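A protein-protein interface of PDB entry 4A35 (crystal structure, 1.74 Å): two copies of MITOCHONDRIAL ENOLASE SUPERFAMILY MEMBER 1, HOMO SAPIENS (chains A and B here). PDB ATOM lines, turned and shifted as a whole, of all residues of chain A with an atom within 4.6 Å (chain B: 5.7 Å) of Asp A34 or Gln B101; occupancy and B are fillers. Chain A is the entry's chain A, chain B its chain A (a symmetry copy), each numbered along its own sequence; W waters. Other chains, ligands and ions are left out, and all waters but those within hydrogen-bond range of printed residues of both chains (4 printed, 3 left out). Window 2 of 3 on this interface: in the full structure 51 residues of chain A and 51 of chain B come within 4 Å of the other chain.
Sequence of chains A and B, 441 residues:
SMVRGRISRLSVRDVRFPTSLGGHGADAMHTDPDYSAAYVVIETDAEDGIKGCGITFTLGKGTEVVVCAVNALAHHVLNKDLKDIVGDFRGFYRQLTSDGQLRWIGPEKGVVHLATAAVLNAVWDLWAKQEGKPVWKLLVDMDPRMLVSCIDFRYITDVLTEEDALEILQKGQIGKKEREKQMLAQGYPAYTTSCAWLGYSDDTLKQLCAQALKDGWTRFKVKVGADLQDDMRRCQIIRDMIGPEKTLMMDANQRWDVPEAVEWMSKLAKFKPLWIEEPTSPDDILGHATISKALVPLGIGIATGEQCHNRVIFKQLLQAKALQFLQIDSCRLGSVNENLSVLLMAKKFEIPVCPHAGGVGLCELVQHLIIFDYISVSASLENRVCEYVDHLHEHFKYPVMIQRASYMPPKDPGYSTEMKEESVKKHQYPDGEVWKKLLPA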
ATOM      1  N   PHE A  17      11.601  14.763   7.044  1.00  0.00           N
ATOM      2  CA  PHE A  17      10.500  15.526   7.600  1.00  0.00           C
ATOM      3  C   PHE A  17      10.814  15.785   9.079  1.00  0.00           C
ATOM      4  O   PHE A  17      11.135  14.856   9.833  1.00  0.00           O
ATOM      5  CB  PHE A  17       9.129  14.834   7.359  1.00  0.00           C
ATOM      6  CG  PHE A  17       8.850  14.630   5.877  1.00  0.00           C
ATOM      7  CD1 PHE A  17       8.224  15.624   5.125  1.00  0.00           C
ATOM      8  CD2 PHE A  17       9.270  13.465   5.223  1.00  0.00           C
ATOM      9  CE1 PHE A  17       8.023  15.469   3.741  1.00  0.00           C
ATOM     10  CE2 PHE A  17       9.070  13.305   3.837  1.00  0.00           C
ATOM     11  CZ  PHE A  17       8.452  14.309   3.106  1.00  0.00           C
ATOM     12  N   PRO A  18      10.591  17.040   9.536  1.00  0.00           N
ATOM     13  CA  PRO A  18      10.930  17.390  10.943  1.00  0.00           C
ATOM     14  C   PRO A  18       9.840  16.977  11.951  1.00  0.00           C
ATOM     15  O   PRO A  18       9.340  17.780  12.731  1.00  0.00           O
ATOM     16  CB  PRO A  18      11.129  18.901  10.884  1.00  0.00           C
ATOM     17  CG  PRO A  18      10.166  19.353   9.735  1.00  0.00           C
ATOM     18  CD  PRO A  18      10.260  18.239   8.719  1.00  0.00           C
ATOM     19  N   THR A  19       9.476  15.713  11.957  1.00  0.00           N
ATOM     20  CA  THR A  19       8.364  15.255  12.801  1.00  0.00           C
ATOM     21  C   THR A  19       8.703  15.344  14.316  1.00  0.00           C
ATOM     22  O   THR A  19       7.768  15.489  15.116  1.00  0.00           O
ATOM     23  CB  THR A  19       7.871  13.881  12.371  1.00  0.00           C
ATOM     24  OG1 THR A  19       8.963  13.034  12.301  1.00  0.00           O
ATOM     25  CG2 THR A  19       7.190  13.893  10.985  1.00  0.00           C
ATOM     26  N   SER A  20      10.011  15.394  14.693  1.00  0.00           N
ATOM     27  CA  SER A  20      10.438  15.525  16.102  1.00  0.00           C
ATOM     28  C   SER A  20       9.981  16.894  16.672  1.00  0.00           C
ATOM     29  O   SER A  20       9.753  17.036  17.887  1.00  0.00           O
ATOM     30  CB  SER A  20      11.954  15.379  16.235  1.00  0.00           C
ATOM     31  OG  SER A  20      12.654  16.435  15.608  1.00  0.00           O
ATOM     32  N   ASP A  32      12.814  10.838  19.534  1.00  0.00           N
ATOM     33  CA  ASP A  32      12.807  12.121  18.780  1.00  0.00           C
ATOM     34  C   ASP A  32      12.974  11.887  17.247  1.00  0.00           C
ATOM     35  O   ASP A  32      13.868  12.487  16.609  1.00  0.00           O
ATOM     36  CB  ASP A  32      13.993  12.984  19.320  1.00  0.00           C
ATOM     37  CG  ASP A  32      15.424  12.456  19.091  1.00  0.00           C
ATOM     38  OD1 ASP A  32      15.591  11.226  18.714  1.00  0.00           O
ATOM     39  OD2 ASP A  32      16.380  13.264  19.221  1.00  0.00           O
ATOM     40  N   PRO A  33      12.156  11.016  16.620  1.00  0.00           N
ATOM     41  CA  PRO A  33      12.435  10.693  15.215  1.00  0.00           C
ATOM     42  C   PRO A  33      12.049  11.842  14.292  1.00  0.00           C
ATOM     43  O   PRO A  33      11.086  12.552  14.540  1.00  0.00           O
ATOM     44  CB  PRO A  33      11.543   9.471  14.959  1.00  0.00           C
ATOM     45  CG  PRO A  33      10.386   9.652  15.897  1.00  0.00           C
ATOM     46  CD  PRO A  33      11.067  10.161  17.150  1.00  0.00           C
ATOM     47  N   ASP A  34      12.791  11.961  13.188  1.00  0.00           N
ATOM     48  CA  ASP A  34      12.475  12.817  12.059  1.00  0.00           C
ATOM     49  C   ASP A  34      12.209  11.838  10.913  1.00  0.00           C
ATOM     50  O   ASP A  34      13.153  11.329  10.283  1.00  0.00           O
ATOM     51  CB  ASP A  34      13.642  13.784  11.751  1.00  0.00           C
ATOM     52  CG  ASP A  34      13.787  14.876  12.792  1.00  0.00           C
ATOM     53  OD1 ASP A  34      12.766  15.438  13.189  1.00  0.00           O
ATOM     54  OD2 ASP A  34      14.953  15.175  13.196  1.00  0.00           O
ATOM     55  N   TYR A  35      10.942  11.526  10.681  1.00  0.00           N
ATOM     56  CA  TYR A  35      10.554  10.583   9.630  1.00  0.00           C
ATOM     57  C   TYR A  35      11.175  11.010   8.310  1.00  0.00           C
ATOM     58  O   TYR A  35      10.945  12.122   7.808  1.00  0.00           O
ATOM     59  CB  TYR A  35       9.024  10.547   9.522  1.00  0.00           C
ATOM     60  CG  TYR A  35       8.312   9.810  10.634  1.00  0.00           C
ATOM     61  CD1 TYR A  35       9.014   9.298  11.732  1.00  0.00           C
ATOM     62  CD2 TYR A  35       6.934   9.624  10.598  1.00  0.00           C
ATOM     63  CE1 TYR A  35       8.351   8.610  12.765  1.00  0.00           C
ATOM     64  CE2 TYR A  35       6.270   8.908  11.603  1.00  0.00           C
ATOM     65  CZ  TYR A  35       6.992   8.366  12.659  1.00  0.00           C
ATOM     66  OH  TYR A  35       6.337   7.681  13.659  1.00  0.00           O
ATOM     67  N   SER A  36      11.930  10.104   7.723  1.00  0.00           N
ATOM     68  CA  SER A  36      12.707  10.388   6.522  1.00  0.00           C
ATOM     69  C   SER A  36      12.718   9.229   5.542  1.00  0.00           C
ATOM     70  O   SER A  36      12.333   8.094   5.885  1.00  0.00           O
ATOM     71  CB  SER A  36      14.153  10.700   6.931  1.00  0.00           C
ATOM     72  OG  SER A  36      14.172  11.826   7.788  1.00  0.00           O
ATOM     73  N   THR A  58      13.598   5.872   7.196  1.00  0.00           N
ATOM     74  CA  THR A  58      14.568   6.067   8.281  1.00  0.00           C
ATOM     75  C   THR A  58      13.993   7.076   9.295  1.00  0.00           C
ATOM     76  O   THR A  58      12.979   7.716   9.028  1.00  0.00           O
ATOM     77  CB  THR A  58      15.975   6.527   7.816  1.00  0.00           C
ATOM     78  OG1 THR A  58      15.876   7.932   7.515  1.00  0.00           O
ATOM     79  CG2 THR A  58      16.565   5.691   6.631  1.00  0.00           C
ATOM     80  N   LEU A  59      14.751   7.292  10.386  1.00  0.00           N
ATOM     81  CA  LEU A  59      14.365   8.238  11.422  1.00  0.00           C
ATOM     82  C   LEU A  59      15.163   9.564  11.366  1.00  0.00           C
ATOM     83  O   LEU A  59      15.110  10.345  12.311  1.00  0.00           O
ATOM     84  CB  LEU A  59      14.516   7.604  12.799  1.00  0.00           C
ATOM     85  CG  LEU A  59      13.679   6.342  13.048  1.00  0.00           C
ATOM     86  CD1 LEU A  59      13.763   5.933  14.534  1.00  0.00           C
ATOM     87  CD2 LEU A  59      12.239   6.528  12.555  1.00  0.00           C
ATOM     88  N   GLY A  60      15.820   9.844  10.254  1.00  0.00           N
ATOM     89  CA  GLY A  60      16.524  11.100  10.087  1.00  0.00           C
ATOM     90  C   GLY A  60      18.004  10.893   9.906  1.00  0.00           C
ATOM     91  O   GLY A  60      18.455  10.610   8.787  1.00  0.00           O
ATOM     92  N   LYS A  61      18.781  10.997  11.009  1.00  0.00           N
ATOM     93  CA  LYS A  61      20.202  10.753  10.899  1.00  0.00           C
ATOM     94  C   LYS A  61      20.416   9.328  10.357  1.00  0.00           C
ATOM     95  O   LYS A  61      19.727   8.407  10.753  1.00  0.00           O
ATOM     96  CB  LYS A  61      20.905  10.911  12.266  1.00  0.00           C
ATOM     97  CG  LYS A  61      20.906  12.364  12.777  1.00  0.00           C
ATOM     98  CD  LYS A  61      21.458  12.338  14.173  1.00  0.00           C
ATOM     99  CE  LYS A  61      21.364  13.619  14.940  1.00  0.00           C
ATOM    100  NZ  LYS A  61      20.251  13.547  15.919  1.00  0.00           N
ATOM    101  N   TRP A 435      15.011  22.610   5.663  1.00  0.00           N
ATOM    102  CA  TRP A 435      16.258  22.393   6.404  1.00  0.00           C
ATOM    103  C   TRP A 435      17.137  23.614   6.402  1.00  0.00           C
ATOM    104  O   TRP A 435      17.880  23.783   7.360  1.00  0.00           O
ATOM    105  CB  TRP A 435      16.978  21.132   5.900  1.00  0.00           C
ATOM    106  CG  TRP A 435      16.119  19.942   6.223  1.00  0.00           C
ATOM    107  CD1 TRP A 435      15.283  19.272   5.367  1.00  0.00           C
ATOM    108  CD2 TRP A 435      15.806  19.467   7.544  1.00  0.00           C
ATOM    109  NE1 TRP A 435      14.506  18.373   6.072  1.00  0.00           N
ATOM    110  CE2 TRP A 435      14.809  18.472   7.409  1.00  0.00           C
ATOM    111  CE3 TRP A 435      16.305  19.764   8.836  1.00  0.00           C
ATOM    112  CZ2 TRP A 435      14.282  17.790   8.511  1.00  0.00           C
ATOM    113  CZ3 TRP A 435      15.731  19.135   9.931  1.00  0.00           C
ATOM    114  CH2 TRP A 435      14.794  18.100   9.754  1.00  0.00           C
ATOM    115  N   ASP B  99      21.731   5.070  19.340  1.00  0.00           N
ATOM    116  CA  ASP B  99      21.414   6.479  19.007  1.00  0.00           C
ATOM    117  C   ASP B  99      19.910   6.491  18.571  1.00  0.00           C
ATOM    118  O   ASP B  99      19.540   5.662  17.761  1.00  0.00           O
ATOM    119  CB  ASP B  99      22.362   6.940  17.880  1.00  0.00           C
ATOM    120  CG  ASP B  99      22.076   8.341  17.354  1.00  0.00           C
ATOM    121  OD1 ASP B  99      21.008   8.541  16.762  1.00  0.00           O
ATOM    122  OD2 ASP B  99      22.957   9.208  17.472  1.00  0.00           O
ATOM    123  N   GLY B 100      19.059   7.336  19.173  1.00  0.00           N
ATOM    124  CA  GLY B 100      17.612   7.345  18.924  1.00  0.00           C
ATOM    125  C   GLY B 100      17.202   7.384  17.464  1.00  0.00           C
ATOM    126  O   GLY B 100      16.148   6.855  17.120  1.00  0.00           O
ATOM    127  N   GLN B 101      18.067   7.944  16.573  1.00  0.00           N
ATOM    128  CA  GLN B 101      17.764   7.920  15.138  1.00  0.00           C
ATOM    129  C   GLN B 101      18.655   6.914  14.384  1.00  0.00           C
ATOM    130  O   GLN B 101      18.125   6.136  13.596  1.00  0.00           O
ATOM    131  CB  GLN B 101      17.911   9.314  14.506  1.00  0.00           C
ATOM    132  CG  GLN B 101      16.882  10.304  15.067  1.00  0.00           C
ATOM    133  CD  GLN B 101      16.857  11.641  14.364  1.00  0.00           C
ATOM    134  OE1 GLN B 101      17.633  11.927  13.461  1.00  0.00           O
ATOM    135  NE2 GLN B 101      15.930  12.499  14.743  1.00  0.00           N
ATOM    136  N   LEU B 102      20.011   6.939  14.607  1.00  0.00           N
ATOM    137  CA  LEU B 102      20.914   6.067  13.848  1.00  0.00           C
ATOM    138  C   LEU B 102      20.662   4.593  14.113  1.00  0.00           C
ATOM    139  O   LEU B 102      20.937   3.784  13.243  1.00  0.00           O
ATOM    140  CB  LEU B 102      22.404   6.392  14.139  1.00  0.00           C
ATOM    141  CG  LEU B 102      22.950   7.637  13.486  1.00  0.00           C
ATOM    142  CD1 LEU B 102      24.372   7.985  14.040  1.00  0.00           C
ATOM    143  CD2 LEU B 102      22.994   7.501  11.951  1.00  0.00           C
ATOM    144  N   ARG B 103      20.125   4.223  15.281  1.00  0.00           N
ATOM    145  CA  ARG B 103      19.938   2.782  15.543  1.00  0.00           C
ATOM    146  C   ARG B 103      18.923   2.157  14.518  1.00  0.00           C
ATOM    147  O   ARG B 103      18.986   0.959  14.238  1.00  0.00           O
ATOM    148  CB  ARG B 103      19.450   2.542  17.005  1.00  0.00           C
ATOM    149  CG  ARG B 103      17.975   2.950  17.226  1.00  0.00           C
ATOM    150  CD  ARG B 103      17.539   2.832  18.704  1.00  0.00           C
ATOM    151  NE  ARG B 103      17.968   1.562  19.311  1.00  0.00           N
ATOM    152  CZ  ARG B 103      17.357   0.392  19.127  1.00  0.00           C
ATOM    153  NH1 ARG B 103      16.284   0.308  18.337  1.00  0.00           N
ATOM    154  NH2 ARG B 103      17.806  -0.698  19.733  1.00  0.00           N
ATOM    155  N   TRP B 104      18.063   2.981  13.926  1.00  0.00           N
ATOM    156  CA  TRP B 104      17.076   2.481  12.956  1.00  0.00           C
ATOM    157  C   TRP B 104      17.785   1.856  11.743  1.00  0.00           C
ATOM    158  O   TRP B 104      17.236   0.935  11.137  1.00  0.00           O
ATOM    159  CB  TRP B 104      16.189   3.639  12.444  1.00  0.00           C
ATOM    160  CG  TRP B 104      14.986   3.166  11.655  1.00  0.00           C
ATOM    161  CD1 TRP B 104      14.868   3.112  10.293  1.00  0.00           C
ATOM    162  CD2 TRP B 104      13.750   2.701  12.184  1.00  0.00           C
ATOM    163  NE1 TRP B 104      13.639   2.607   9.947  1.00  0.00           N
ATOM    164  CE2 TRP B 104      12.913   2.386  11.086  1.00  0.00           C
ATOM    165  CE3 TRP B 104      13.255   2.519  13.496  1.00  0.00           C
ATOM    166  CZ2 TRP B 104      11.648   1.806  11.254  1.00  0.00           C
ATOM    167  CZ3 TRP B 104      11.974   2.016  13.665  1.00  0.00           C
ATOM    168  CH2 TRP B 104      11.166   1.702  12.550  1.00  0.00           C
ATOM    169  N   ILE B 105      18.986   2.363  11.400  1.00  0.00           N
ATOM    170  CA  ILE B 105      19.679   1.821  10.233  1.00  0.00           C
ATOM    171  C   ILE B 105      20.464   0.509  10.559  1.00  0.00           C
ATOM    172  O   ILE B 105      21.052  -0.081   9.645  1.00  0.00           O
ATOM    173  CB  ILE B 105      20.496   2.831   9.457  1.00  0.00           C
ATOM    174  CG1 ILE B 105      21.729   3.297  10.262  1.00  0.00           C
ATOM    175  CG2 ILE B 105      19.577   4.015   8.943  1.00  0.00           C
ATOM    176  CD1 ILE B 105      22.748   4.200   9.357  1.00  0.00           C
HETATM  177  O   HOH W   1      18.195  10.657  19.075  1.00  0.00           O
HETATM  178  O   HOH W   2      14.257   8.977  17.561  1.00  0.00           O
HETATM  179  O   HOH W   3      19.918  10.929  17.148  1.00  0.00           O
HETATM  180  O   HOH W   4      17.517   6.564  10.962  1.00  0.00           O
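NE2 of Gln B101 sits at hydrogen-bond distance from O of Asp A32 (2.8 Å).
OD2 of Asp A34 lies within hydrogen-bond range of NE2 of Gln B101 (3.2 Å).
The backbone carbonyl oxygen of Leu A59 sits close to the side-chain amide oxygen of Gln B101, at 3.2 Å.
N of Lys A61 lies within hydrogen-bond range of OE1 of Gln B101, at 2.9 Å.
Of the 7 printed residues of chain B, 4 touch a printed residue of chain A.
Printed residues of chain B that touch a printed residue of chain A: Gly B100, Gln B101, Leu B102 and Trp B104.
Hydrophobic or aromatic side chains of chain B within 4 Å of the printed part of chain A: Leu B102 and Trp B104.
Of the 14 printed residues of chain A, 7 touch a printed residue of chain B.
Hydrophobic or aromatic side chains of chain A within 4 Å of the printed part of chain B: Leu A59.
Along chain A the printed residues that touch a printed residue of chain B span positions 32 to 61.
Among the printed residues, 10 pairs touch across the chains.
Among the printed residues, pairs that only touch across the chains: Pro A33 with Gln B101 (3.96 Å), Thr A58 with Trp B104 (3.6 Å), Leu A59 with Gly B100 (3.6 Å), Leu A59 with Trp B104 (3.6 Å), Gly A60 with Gln B101 (3.6 Å) and Lys A61 with Leu B102 (3.5 Å).
No position is printed for both chains.
The backbone carbonyl oxygen of Pro A33 sits at hydrogen-bond distance from the side-chain hydroxyl of Thr A19 (3.1 Å).
The backbone carbonyl oxygen (O) of Pro A33 sits at hydrogen-bond distance from the backbone NH (N) of Ser A20.
The backbone carbonyl oxygen (O) of Asp A34 is in hydrogen-bond range of the backbone NH (N) of Gly A60 (3.1 Å).
The backbone NH of Thr A58 sits at hydrogen-bond distance from the backbone carbonyl oxygen of Ser A36.
OD1 of Asp B99 lies within hydrogen-bond range of N of Gln B101 (3.0 Å).
OD1 of Asp B99 sits at hydrogen-bond distance from N of Leu B102 (2.9 Å).
Of chain B, only Gln B101 (3.2 Å) comes within 4 Å of Asp A34.
Of the printed residues of chain B, Leu A59 touches Gly B100, Gln B101 and Trp B104.
Of the printed residues of chain B, Lys A61 touches Gln B101 (2.9 Å) and Leu B102 (3.5 Å).
Gln B101 touches six residues of chain A.
Of the printed residues of chain A, Leu B102 touches Lys A61.
Printed residues of chain A within 4 Å of Trp B104: Thr A58 and Leu A59.
Water W3 bridges OD1 of Asp B99 and NZ of Lys A61.
Water W1 lies within hydrogen-bond range of OD1 of Asp A32 and N of Gly B100.
Water W4 lies within hydrogen-bond range of O of Gln B101 (2.7 Å), O of Lys A61 (2.9 Å) and N of Leu A59 (2.9 Å).
Water W2 lies within hydrogen-bond range of OD1 of Asp A32 and O of Gly B100.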
